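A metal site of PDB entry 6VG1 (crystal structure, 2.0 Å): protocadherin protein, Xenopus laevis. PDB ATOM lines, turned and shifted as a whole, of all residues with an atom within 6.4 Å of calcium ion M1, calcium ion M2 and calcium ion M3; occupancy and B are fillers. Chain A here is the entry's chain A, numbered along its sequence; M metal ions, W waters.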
ATOM      1  N   GLU A   9      20.304  12.368 -14.690  1.00  0.00           N
ATOM      2  CA  GLU A   9      19.065  13.132 -14.702  1.00  0.00           C
ATOM      3  C   GLU A   9      18.157  12.690 -15.848  1.00  0.00           C
ATOM      4  O   GLU A   9      18.615  12.110 -16.833  1.00  0.00           O
ATOM      5  CB  GLU A   9      19.355  14.637 -14.811  1.00  0.00           C
ATOM      6  CG  GLU A   9      19.910  15.091 -16.141  1.00  0.00           C
ATOM      7  CD  GLU A   9      19.843  16.601 -16.329  1.00  0.00           C
ATOM      8  OE1 GLU A   9      18.816  17.206 -15.929  1.00  0.00           O
ATOM      9  OE2 GLU A   9      20.807  17.199 -16.865  1.00  0.00           O
ATOM     10  N   GLU A  10      16.857  12.951 -15.706  1.00  0.00           N
ATOM     11  CA  GLU A  10      15.868  12.645 -16.732  1.00  0.00           C
ATOM     12  C   GLU A  10      15.933  11.174 -17.161  1.00  0.00           C
ATOM     13  O   GLU A  10      15.761  10.849 -18.335  1.00  0.00           O
ATOM     14  CB  GLU A  10      16.029  13.552 -17.958  1.00  0.00           C
ATOM     15  CG  GLU A  10      16.417  14.990 -17.695  1.00  0.00           C
ATOM     16  CD  GLU A  10      15.241  15.963 -17.803  1.00  0.00           C
ATOM     17  OE1 GLU A  10      14.081  15.523 -17.727  1.00  0.00           O
ATOM     18  OE2 GLU A  10      15.510  17.176 -17.955  1.00  0.00           O
ATOM     19  N   ARG A  57      10.077  12.335 -12.471  1.00  0.00           N
ATOM     20  CA  ARG A  57      11.070  12.936 -13.351  1.00  0.00           C
ATOM     21  C   ARG A  57      12.113  13.687 -12.543  1.00  0.00           C
ATOM     22  O   ARG A  57      11.780  14.410 -11.594  1.00  0.00           O
ATOM     23  CB  ARG A  57      10.362  13.865 -14.323  1.00  0.00           C
ATOM     24  CG  ARG A  57      11.245  14.565 -15.327  1.00  0.00           C
ATOM     25  CD  ARG A  57      10.369  15.445 -16.219  1.00  0.00           C
ATOM     26  NE  ARG A  57      11.122  16.186 -17.223  1.00  0.00           N
ATOM     27  CZ  ARG A  57      11.631  17.390 -17.018  1.00  0.00           C
ATOM     28  NH1 ARG A  57      11.484  18.002 -15.855  1.00  0.00           N
ATOM     29  NH2 ARG A  57      12.291  18.002 -17.995  1.00  0.00           N
ATOM     30  N   ILE A  58      13.377  13.516 -12.913  1.00  0.00           N
ATOM     31  CA  ILE A  58      14.494  14.161 -12.228  1.00  0.00           C
ATOM     32  C   ILE A  58      15.198  15.084 -13.220  1.00  0.00           C
ATOM     33  O   ILE A  58      15.936  14.605 -14.086  1.00  0.00           O
ATOM     34  CB  ILE A  58      15.484  13.152 -11.642  1.00  0.00           C
ATOM     35  CG1 ILE A  58      14.810  12.271 -10.597  1.00  0.00           C
ATOM     36  CG2 ILE A  58      16.685  13.881 -11.044  1.00  0.00           C
ATOM     37  CD1 ILE A  58      15.683  11.121 -10.118  1.00  0.00           C
ATOM     38  N   ASP A  59      14.978  16.396 -13.084  1.00  0.00           N
ATOM     39  CA  ASP A  59      15.598  17.395 -13.954  1.00  0.00           C
ATOM     40  C   ASP A  59      16.624  18.183 -13.154  1.00  0.00           C
ATOM     41  O   ASP A  59      16.262  19.020 -12.322  1.00  0.00           O
ATOM     42  CB  ASP A  59      14.534  18.321 -14.543  1.00  0.00           C
ATOM     43  CG  ASP A  59      15.102  19.278 -15.589  1.00  0.00           C
ATOM     44  OD1 ASP A  59      16.318  19.205 -15.878  1.00  0.00           O
ATOM     45  OD2 ASP A  59      14.331  20.097 -16.130  1.00  0.00           O
ATOM     46  N   ARG A  60      17.906  17.941 -13.437  1.00  0.00           N
ATOM     47  CA  ARG A  60      18.963  18.618 -12.682  1.00  0.00           C
ATOM     48  C   ARG A  60      18.839  20.134 -12.806  1.00  0.00           C
ATOM     49  O   ARG A  60      18.941  20.858 -11.815  1.00  0.00           O
ATOM     50  CB  ARG A  60      20.335  18.158 -13.161  1.00  0.00           C
ATOM     51  CG  ARG A  60      21.444  18.392 -12.139  1.00  0.00           C
ATOM     52  CD  ARG A  60      22.787  18.633 -12.785  1.00  0.00           C
ATOM     53  NE  ARG A  60      22.714  19.714 -13.774  1.00  0.00           N
ATOM     54  CZ  ARG A  60      22.511  20.994 -13.477  1.00  0.00           C
ATOM     55  NH1 ARG A  60      22.357  21.358 -12.213  1.00  0.00           N
ATOM     56  NH2 ARG A  60      22.468  21.896 -14.439  1.00  0.00           N
ATOM     57  N   GLU A  61      18.628  20.630 -14.021  1.00  0.00           N
ATOM     58  CA  GLU A  61      18.558  22.068 -14.245  1.00  0.00           C
ATOM     59  C   GLU A  61      17.403  22.727 -13.487  1.00  0.00           C
ATOM     60  O   GLU A  61      17.401  23.958 -13.357  1.00  0.00           O
ATOM     61  CB  GLU A  61      18.440  22.353 -15.742  1.00  0.00           C
ATOM     62  CG  GLU A  61      19.756  22.215 -16.534  1.00  0.00           C
ATOM     63  CD  GLU A  61      20.080  20.796 -16.946  1.00  0.00           C
ATOM     64  OE1 GLU A  61      19.196  20.090 -17.476  1.00  0.00           O
ATOM     65  OE2 GLU A  61      21.237  20.378 -16.747  1.00  0.00           O
ATOM     66  N   ARG A  62      16.448  21.951 -12.970  1.00  0.00           N
ATOM     67  CA  ARG A  62      15.330  22.499 -12.216  1.00  0.00           C
ATOM     68  C   ARG A  62      15.544  22.452 -10.713  1.00  0.00           C
ATOM     69  O   ARG A  62      14.964  23.268  -9.993  1.00  0.00           O
ATOM     70  CB  ARG A  62      14.036  21.759 -12.556  1.00  0.00           C
ATOM     71  CG  ARG A  62      12.841  22.205 -11.731  1.00  0.00           C
ATOM     72  CD  ARG A  62      11.553  21.506 -12.173  1.00  0.00           C
ATOM     73  NE  ARG A  62      11.641  20.053 -12.023  1.00  0.00           N
ATOM     74  CZ  ARG A  62      11.430  19.398 -10.888  1.00  0.00           C
ATOM     75  NH1 ARG A  62      11.135  20.064  -9.781  1.00  0.00           N
ATOM     76  NH2 ARG A  62      11.531  18.079 -10.855  1.00  0.00           N
ATOM     77  N   ASP A  95      24.927  15.263 -14.705  1.00  0.00           N
ATOM     78  CA  ASP A  95      24.358  16.205 -15.658  1.00  0.00           C
ATOM     79  C   ASP A  95      24.362  15.600 -17.061  1.00  0.00           C
ATOM     80  O   ASP A  95      25.327  14.952 -17.470  1.00  0.00           O
ATOM     81  CB  ASP A  95      25.137  17.517 -15.655  1.00  0.00           C
ATOM     82  CG  ASP A  95      24.637  18.505 -16.698  1.00  0.00           C
ATOM     83  OD1 ASP A  95      23.589  18.254 -17.335  1.00  0.00           O
ATOM     84  OD2 ASP A  95      25.297  19.551 -16.893  1.00  0.00           O
ATOM     85  N   ILE A  96      23.266  15.845 -17.793  1.00  0.00           N
ATOM     86  CA  ILE A  96      23.136  15.456 -19.190  1.00  0.00           C
ATOM     87  C   ILE A  96      23.081  16.726 -20.017  1.00  0.00           C
ATOM     88  O   ILE A  96      22.666  17.784 -19.530  1.00  0.00           O
ATOM     89  CB  ILE A  96      21.902  14.568 -19.410  1.00  0.00           C
ATOM     90  CG1 ILE A  96      22.086  13.694 -20.651  1.00  0.00           C
ATOM     91  CG2 ILE A  96      20.644  15.402 -19.561  1.00  0.00           C
ATOM     92  CD1 ILE A  96      23.188  12.652 -20.510  1.00  0.00           C
ATOM     93  N   ASN A  97      23.502  16.615 -21.277  1.00  0.00           N
ATOM     94  CA  ASN A  97      23.633  17.776 -22.160  1.00  0.00           C
ATOM     95  C   ASN A  97      22.339  18.037 -22.937  1.00  0.00           C
ATOM     96  O   ASN A  97      22.325  18.149 -24.162  1.00  0.00           O
ATOM     97  CB  ASN A  97      24.802  17.541 -23.104  1.00  0.00           C
ATOM     98  CG  ASN A  97      25.212  18.804 -23.846  1.00  0.00           C
ATOM     99  OD1 ASN A  97      25.031  19.918 -23.343  1.00  0.00           O
ATOM    100  ND2 ASN A  97      25.754  18.634 -25.043  1.00  0.00           N
ATOM    101  N   ASP A  98      21.240  18.142 -22.196  1.00  0.00           N
ATOM    102  CA  ASP A  98      19.923  18.365 -22.780  1.00  0.00           C
ATOM    103  C   ASP A  98      19.582  19.838 -22.902  1.00  0.00           C
ATOM    104  O   ASP A  98      18.413  20.180 -23.069  1.00  0.00           O
ATOM    105  CB  ASP A  98      18.847  17.648 -21.949  1.00  0.00           C
ATOM    106  CG  ASP A  98      18.950  17.949 -20.453  1.00  0.00           C
ATOM    107  OD1 ASP A  98      19.891  18.660 -20.028  1.00  0.00           O
ATOM    108  OD2 ASP A  98      18.084  17.450 -19.705  1.00  0.00           O
ATOM    109  N   ASN A  99      20.582  20.714 -22.840  1.00  0.00           N
ATOM    110  CA  ASN A  99      20.361  22.136 -23.048  1.00  0.00           C
ATOM    111  C   ASN A  99      21.477  22.688 -23.905  1.00  0.00           C
ATOM    112  O   ASN A  99      22.663  22.385 -23.682  1.00  0.00           O
ATOM    113  CB  ASN A  99      20.285  22.900 -21.727  1.00  0.00           C
ATOM    114  CG  ASN A  99      18.935  22.763 -21.057  1.00  0.00           C
ATOM    115  OD1 ASN A  99      17.911  23.172 -21.617  1.00  0.00           O
ATOM    116  ND2 ASN A  99      18.906  22.178 -19.873  1.00  0.00           N
ATOM    117  N   SER A 100      21.089  23.526 -24.879  1.00  0.00           N
ATOM    118  CA  SER A 100      21.988  24.106 -25.838  1.00  0.00           C
ATOM    119  C   SER A 100      22.186  25.581 -25.554  1.00  0.00           C
ATOM    120  O   SER A 100      21.298  26.240 -25.008  1.00  0.00           O
ATOM    121  CB  SER A 100      21.410  23.923 -27.230  1.00  0.00           C
ATOM    122  OG  SER A 100      20.012  24.213 -27.220  1.00  0.00           O
ATOM    123  N   PRO A 101      23.321  26.136 -25.953  1.00  0.00           N
ATOM    124  CA  PRO A 101      23.533  27.586 -25.766  1.00  0.00           C
ATOM    125  C   PRO A 101      22.432  28.387 -26.433  1.00  0.00           C
ATOM    126  O   PRO A 101      21.981  28.065 -27.531  1.00  0.00           O
ATOM    127  CB  PRO A 101      24.898  27.835 -26.407  1.00  0.00           C
ATOM    128  CG  PRO A 101      25.603  26.506 -26.350  1.00  0.00           C
ATOM    129  CD  PRO A 101      24.504  25.463 -26.530  1.00  0.00           C
ATOM    130  N   ASP A 129      23.892  28.549 -21.315  1.00  0.00           N
ATOM    131  CA  ASP A 129      23.670  27.109 -21.432  1.00  0.00           C
ATOM    132  C   ASP A 129      23.340  26.610 -20.039  1.00  0.00           C
ATOM    133  O   ASP A 129      24.177  26.714 -19.133  1.00  0.00           O
ATOM    134  CB  ASP A 129      24.903  26.402 -21.990  1.00  0.00           C
ATOM    135  CG  ASP A 129      24.655  24.924 -22.290  1.00  0.00           C
ATOM    136  OD1 ASP A 129      23.618  24.337 -21.888  1.00  0.00           O
ATOM    137  OD2 ASP A 129      25.556  24.326 -22.925  1.00  0.00           O
ATOM    138  N   GLU A 130      22.125  26.091 -19.853  1.00  0.00           N
ATOM    139  CA  GLU A 130      21.654  25.750 -18.518  1.00  0.00           C
ATOM    140  C   GLU A 130      22.291  24.476 -17.961  1.00  0.00           C
ATOM    141  O   GLU A 130      21.989  24.131 -16.815  1.00  0.00           O
ATOM    142  CB  GLU A 130      20.125  25.616 -18.530  1.00  0.00           C
ATOM    143  CG  GLU A 130      19.416  26.942 -18.749  1.00  0.00           C
ATOM    144  CD  GLU A 130      17.922  26.855 -18.493  1.00  0.00           C
ATOM    145  OE1 GLU A 130      17.418  25.724 -18.316  1.00  0.00           O
ATOM    146  OE2 GLU A 130      17.259  27.912 -18.471  1.00  0.00           O
ATOM    147  N   ASP A 131      23.127  23.784 -18.722  1.00  0.00           N
ATOM    148  CA  ASP A 131      23.914  22.685 -18.170  1.00  0.00           C
ATOM    149  C   ASP A 131      25.083  23.248 -17.370  1.00  0.00           C
ATOM    150  O   ASP A 131      25.215  24.472 -17.202  1.00  0.00           O
ATOM    151  CB  ASP A 131      24.380  21.775 -19.302  1.00  0.00           C
ATOM    152  CG  ASP A 131      23.230  21.293 -20.178  1.00  0.00           C
ATOM    153  OD1 ASP A 131      22.133  20.973 -19.646  1.00  0.00           O
ATOM    154  OD2 ASP A 131      23.419  21.237 -21.422  1.00  0.00           O
ATOM    155  N   VAL A 132      25.944  22.366 -16.852  1.00  0.00           N
ATOM    156  CA  VAL A 132      27.107  22.797 -16.088  1.00  0.00           C
ATOM    157  C   VAL A 132      28.350  22.084 -16.618  1.00  0.00           C
ATOM    158  O   VAL A 132      28.263  21.171 -17.438  1.00  0.00           O
ATOM    159  CB  VAL A 132      26.943  22.528 -14.564  1.00  0.00           C
ATOM    160  CG1 VAL A 132      25.785  23.330 -13.991  1.00  0.00           C
ATOM    161  CG2 VAL A 132      26.753  21.043 -14.313  1.00  0.00           C
ATOM    162  N   VAL A 134      31.541  20.814 -18.519  1.00  0.00           N
ATOM    163  CA  VAL A 134      31.828  20.803 -19.950  1.00  0.00           C
ATOM    164  C   VAL A 134      30.564  21.066 -20.749  1.00  0.00           C
ATOM    165  O   VAL A 134      30.608  21.644 -21.842  1.00  0.00           O
ATOM    166  CB  VAL A 134      32.484  19.480 -20.371  1.00  0.00           C
ATOM    167  CG1 VAL A 134      33.736  19.226 -19.555  1.00  0.00           C
ATOM    168  CG2 VAL A 134      31.483  18.329 -20.252  1.00  0.00           C
ATOM    169  N   ASN A 135      29.409  20.639 -20.230  1.00  0.00           N
ATOM    170  CA  ASN A 135      28.141  20.872 -20.915  1.00  0.00           C
ATOM    171  C   ASN A 135      27.734  22.336 -20.918  1.00  0.00           C
ATOM    172  O   ASN A 135      26.706  22.673 -21.514  1.00  0.00           O
ATOM    173  CB  ASN A 135      27.045  20.029 -20.287  1.00  0.00           C
ATOM    174  CG  ASN A 135      27.255  18.549 -20.521  1.00  0.00           C
ATOM    175  OD1 ASN A 135      28.139  18.166 -21.288  1.00  0.00           O
ATOM    176  ND2 ASN A 135      26.448  17.722 -19.872  1.00  0.00           N
ATOM    177  N   SER A 136      28.518  23.202 -20.287  1.00  0.00           N
ATOM    178  CA  SER A 136      28.282  24.641 -20.312  1.00  0.00           C
ATOM    179  C   SER A 136      29.001  25.253 -21.515  1.00  0.00           C
ATOM    180  O   SER A 136      29.746  24.577 -22.242  1.00  0.00           O
ATOM    181  CB  SER A 136      28.755  25.285 -19.025  1.00  0.00           C
ATOM    182  OG  SER A 136      30.180  25.322 -18.975  1.00  0.00           O
ATOM    183  N   ILE A 137      28.806  26.546 -21.726  1.00  0.00           N
ATOM    184  CA  ILE A 137      29.416  27.237 -22.863  1.00  0.00           C
ATOM    185  C   ILE A 137      30.924  27.256 -22.674  1.00  0.00           C
ATOM    186  O   ILE A 137      31.435  27.789 -21.682  1.00  0.00           O
ATOM    187  CB  ILE A 137      28.857  28.655 -22.996  1.00  0.00           C
ATOM    188  CG1 ILE A 137      27.375  28.586 -23.379  1.00  0.00           C
ATOM    189  CG2 ILE A 137      29.640  29.448 -24.043  1.00  0.00           C
ATOM    190  CD1 ILE A 137      26.661  29.935 -23.375  1.00  0.00           C
ATOM    191  N   ASP A 186      29.304  24.292 -26.510  1.00  0.00           N
ATOM    192  CA  ASP A 186      29.703  23.638 -25.275  1.00  0.00           C
ATOM    193  C   ASP A 186      30.608  22.438 -25.563  1.00  0.00           C
ATOM    194  O   ASP A 186      30.884  22.090 -26.716  1.00  0.00           O
ATOM    195  CB  ASP A 186      28.461  23.210 -24.477  1.00  0.00           C
ATOM    196  CG  ASP A 186      27.561  22.225 -25.244  1.00  0.00           C
ATOM    197  OD1 ASP A 186      28.073  21.464 -26.102  1.00  0.00           O
ATOM    198  OD2 ASP A 186      26.340  22.215 -24.981  1.00  0.00           O
ATOM    199  N   GLY A 187      31.045  21.777 -24.483  1.00  0.00           N
ATOM    200  CA  GLY A 187      31.984  20.681 -24.588  1.00  0.00           C
ATOM    201  C   GLY A 187      31.312  19.325 -24.767  1.00  0.00           C
ATOM    202  O   GLY A 187      30.081  19.201 -24.784  1.00  0.00           O
ATOM    203  N   ARG A 192      26.526  21.148 -28.781  1.00  0.00           N
ATOM    204  CA  ARG A 192      25.354  21.938 -29.123  1.00  0.00           C
ATOM    205  C   ARG A 192      25.758  23.400 -29.259  1.00  0.00           C
ATOM    206  O   ARG A 192      26.393  23.964 -28.358  1.00  0.00           O
ATOM    207  CB  ARG A 192      24.254  21.761 -28.084  1.00  0.00           C
ATOM    208  CG  ARG A 192      23.687  20.337 -28.088  1.00  0.00           C
ATOM    209  CD  ARG A 192      22.965  19.975 -26.799  1.00  0.00           C
ATOM    210  NE  ARG A 192      21.622  20.536 -26.698  1.00  0.00           N
ATOM    211  CZ  ARG A 192      20.505  19.837 -26.853  1.00  0.00           C
ATOM    212  NH1 ARG A 192      20.553  18.544 -27.121  1.00  0.00           N
ATOM    213  NH2 ARG A 192      19.327  20.441 -26.725  1.00  0.00           N
HETATM  214 CA    CA M   1      24.886  22.228 -22.904  1.00  0.00          CA
HETATM  215 CA    CA M   2      21.553  18.981 -18.350  1.00  0.00          CA
HETATM  216 CA    CA M   3      17.645  18.360 -17.697  1.00  0.00          CA
HETATM  217  O   HOH W   1      15.556  20.087 -18.828  1.00  0.00           O
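The backbone carbonyl oxygen (O) of Asn 97 sits close to the guanidinium group (NH1) of Arg 192 (3.5 Å).
The side-chain carboxylate of Asp 95 sits at hydrogen-bond distance from the backbone NH of Val 132, 2.9 Å away.
The side-chain carboxylate (OD2) of Asp 59 is in salt-bridge range of the guanidinium group (NH2) of Arg 57, 3.5 Å away.
OE2 of Glu 61 lies close to NH2 of Arg 60, at 3.0 Å.
The side-chain carboxylate of Glu 61 lies close to the side-chain amide nitrogen of Asn 99.
The guanidinium group (NH2) of Arg 57 is in salt-bridge range of the side-chain carboxylate (OE1) of Glu 10, at 3.1 Å.
OD1 of Asp 95 lies close to NE of Arg 60, 3.9 Å away.
N of Glu 10 is in hydrogen-bond range of O of Ile 58 (2.5 Å).
Within 4 Å of calcium ion M1: Asn 97, Asn 99, Asp 129, Asp 131, Asn 135 and Asp 186.
Six residues have an atom within 4 Å of calcium ion M2: Glu 9, Glu 61, Asp 95, Ile 96, Asp 98 and Asp 131.
The nearest printed residue that does not touch calcium ion M2 is Asn 97 (4.2 Å).
Of the 26 residues printed, 5 come within 4 Å of calcium ion M3.
The nearest printed residue that does not touch calcium ion M3 is Arg 60 (4.3 Å).
OD2 of Asp 129 binds calcium ion M1.
Calcium ion M1 is bound by OD2 of Asp 131 (2.3 Å).
O of Asn 135 binds calcium ion M1 (2.3 Å).
Calcium ion M1 is bound by OD1 of Asn 97, 2.4 Å away.
O of Asn 99 binds calcium ion M1, at 2.4 Å.
Calcium ion M1 is bound by OD2 of Asp 186.
The side-chain carboxylate (OD1) of Asp 129 is bound to calcium ion M1 (2.7 Å).
Calcium ion M1 has seven donor atoms within binding distance.
O of Ile 96 is bound to calcium ion M2, 2.0 Å away.
Calcium ion M2 is bound by OE2 of Glu 61, 2.1 Å away.
The side-chain carboxylate (OD1) of Asp 98 binds calcium ion M2, 2.4 Å away.
Calcium ion M2 is bound by OD1 of Asp 95, at 2.4 Å.
OE2 of Glu 9 binds calcium ion M2 (2.4 Å).
Calcium ion M2 is bound by OD1 of Asp 131 (2.4 Å).
Calcium ion M2 is bound by OE1 of Glu 61, 2.7 Å away.
OD2 of Asp 98 binds calcium ion M3 (2.2 Å).
OE1 of Glu 61 is bound to calcium ion M3 (2.3 Å).
OD1 of Asp 59 binds calcium ion M3 (2.4 Å).
Calcium ion M3 is bound by the side-chain carboxylate (OE1) of Glu 9 (2.4 Å).
Calcium ion M3 is bound by OE2 of Glu 10, at 2.5 Å.
Calcium ion M3 has five donor atoms within binding distance.
Slightly farther from calcium ion M3 lies water W1 (2.9 Å).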
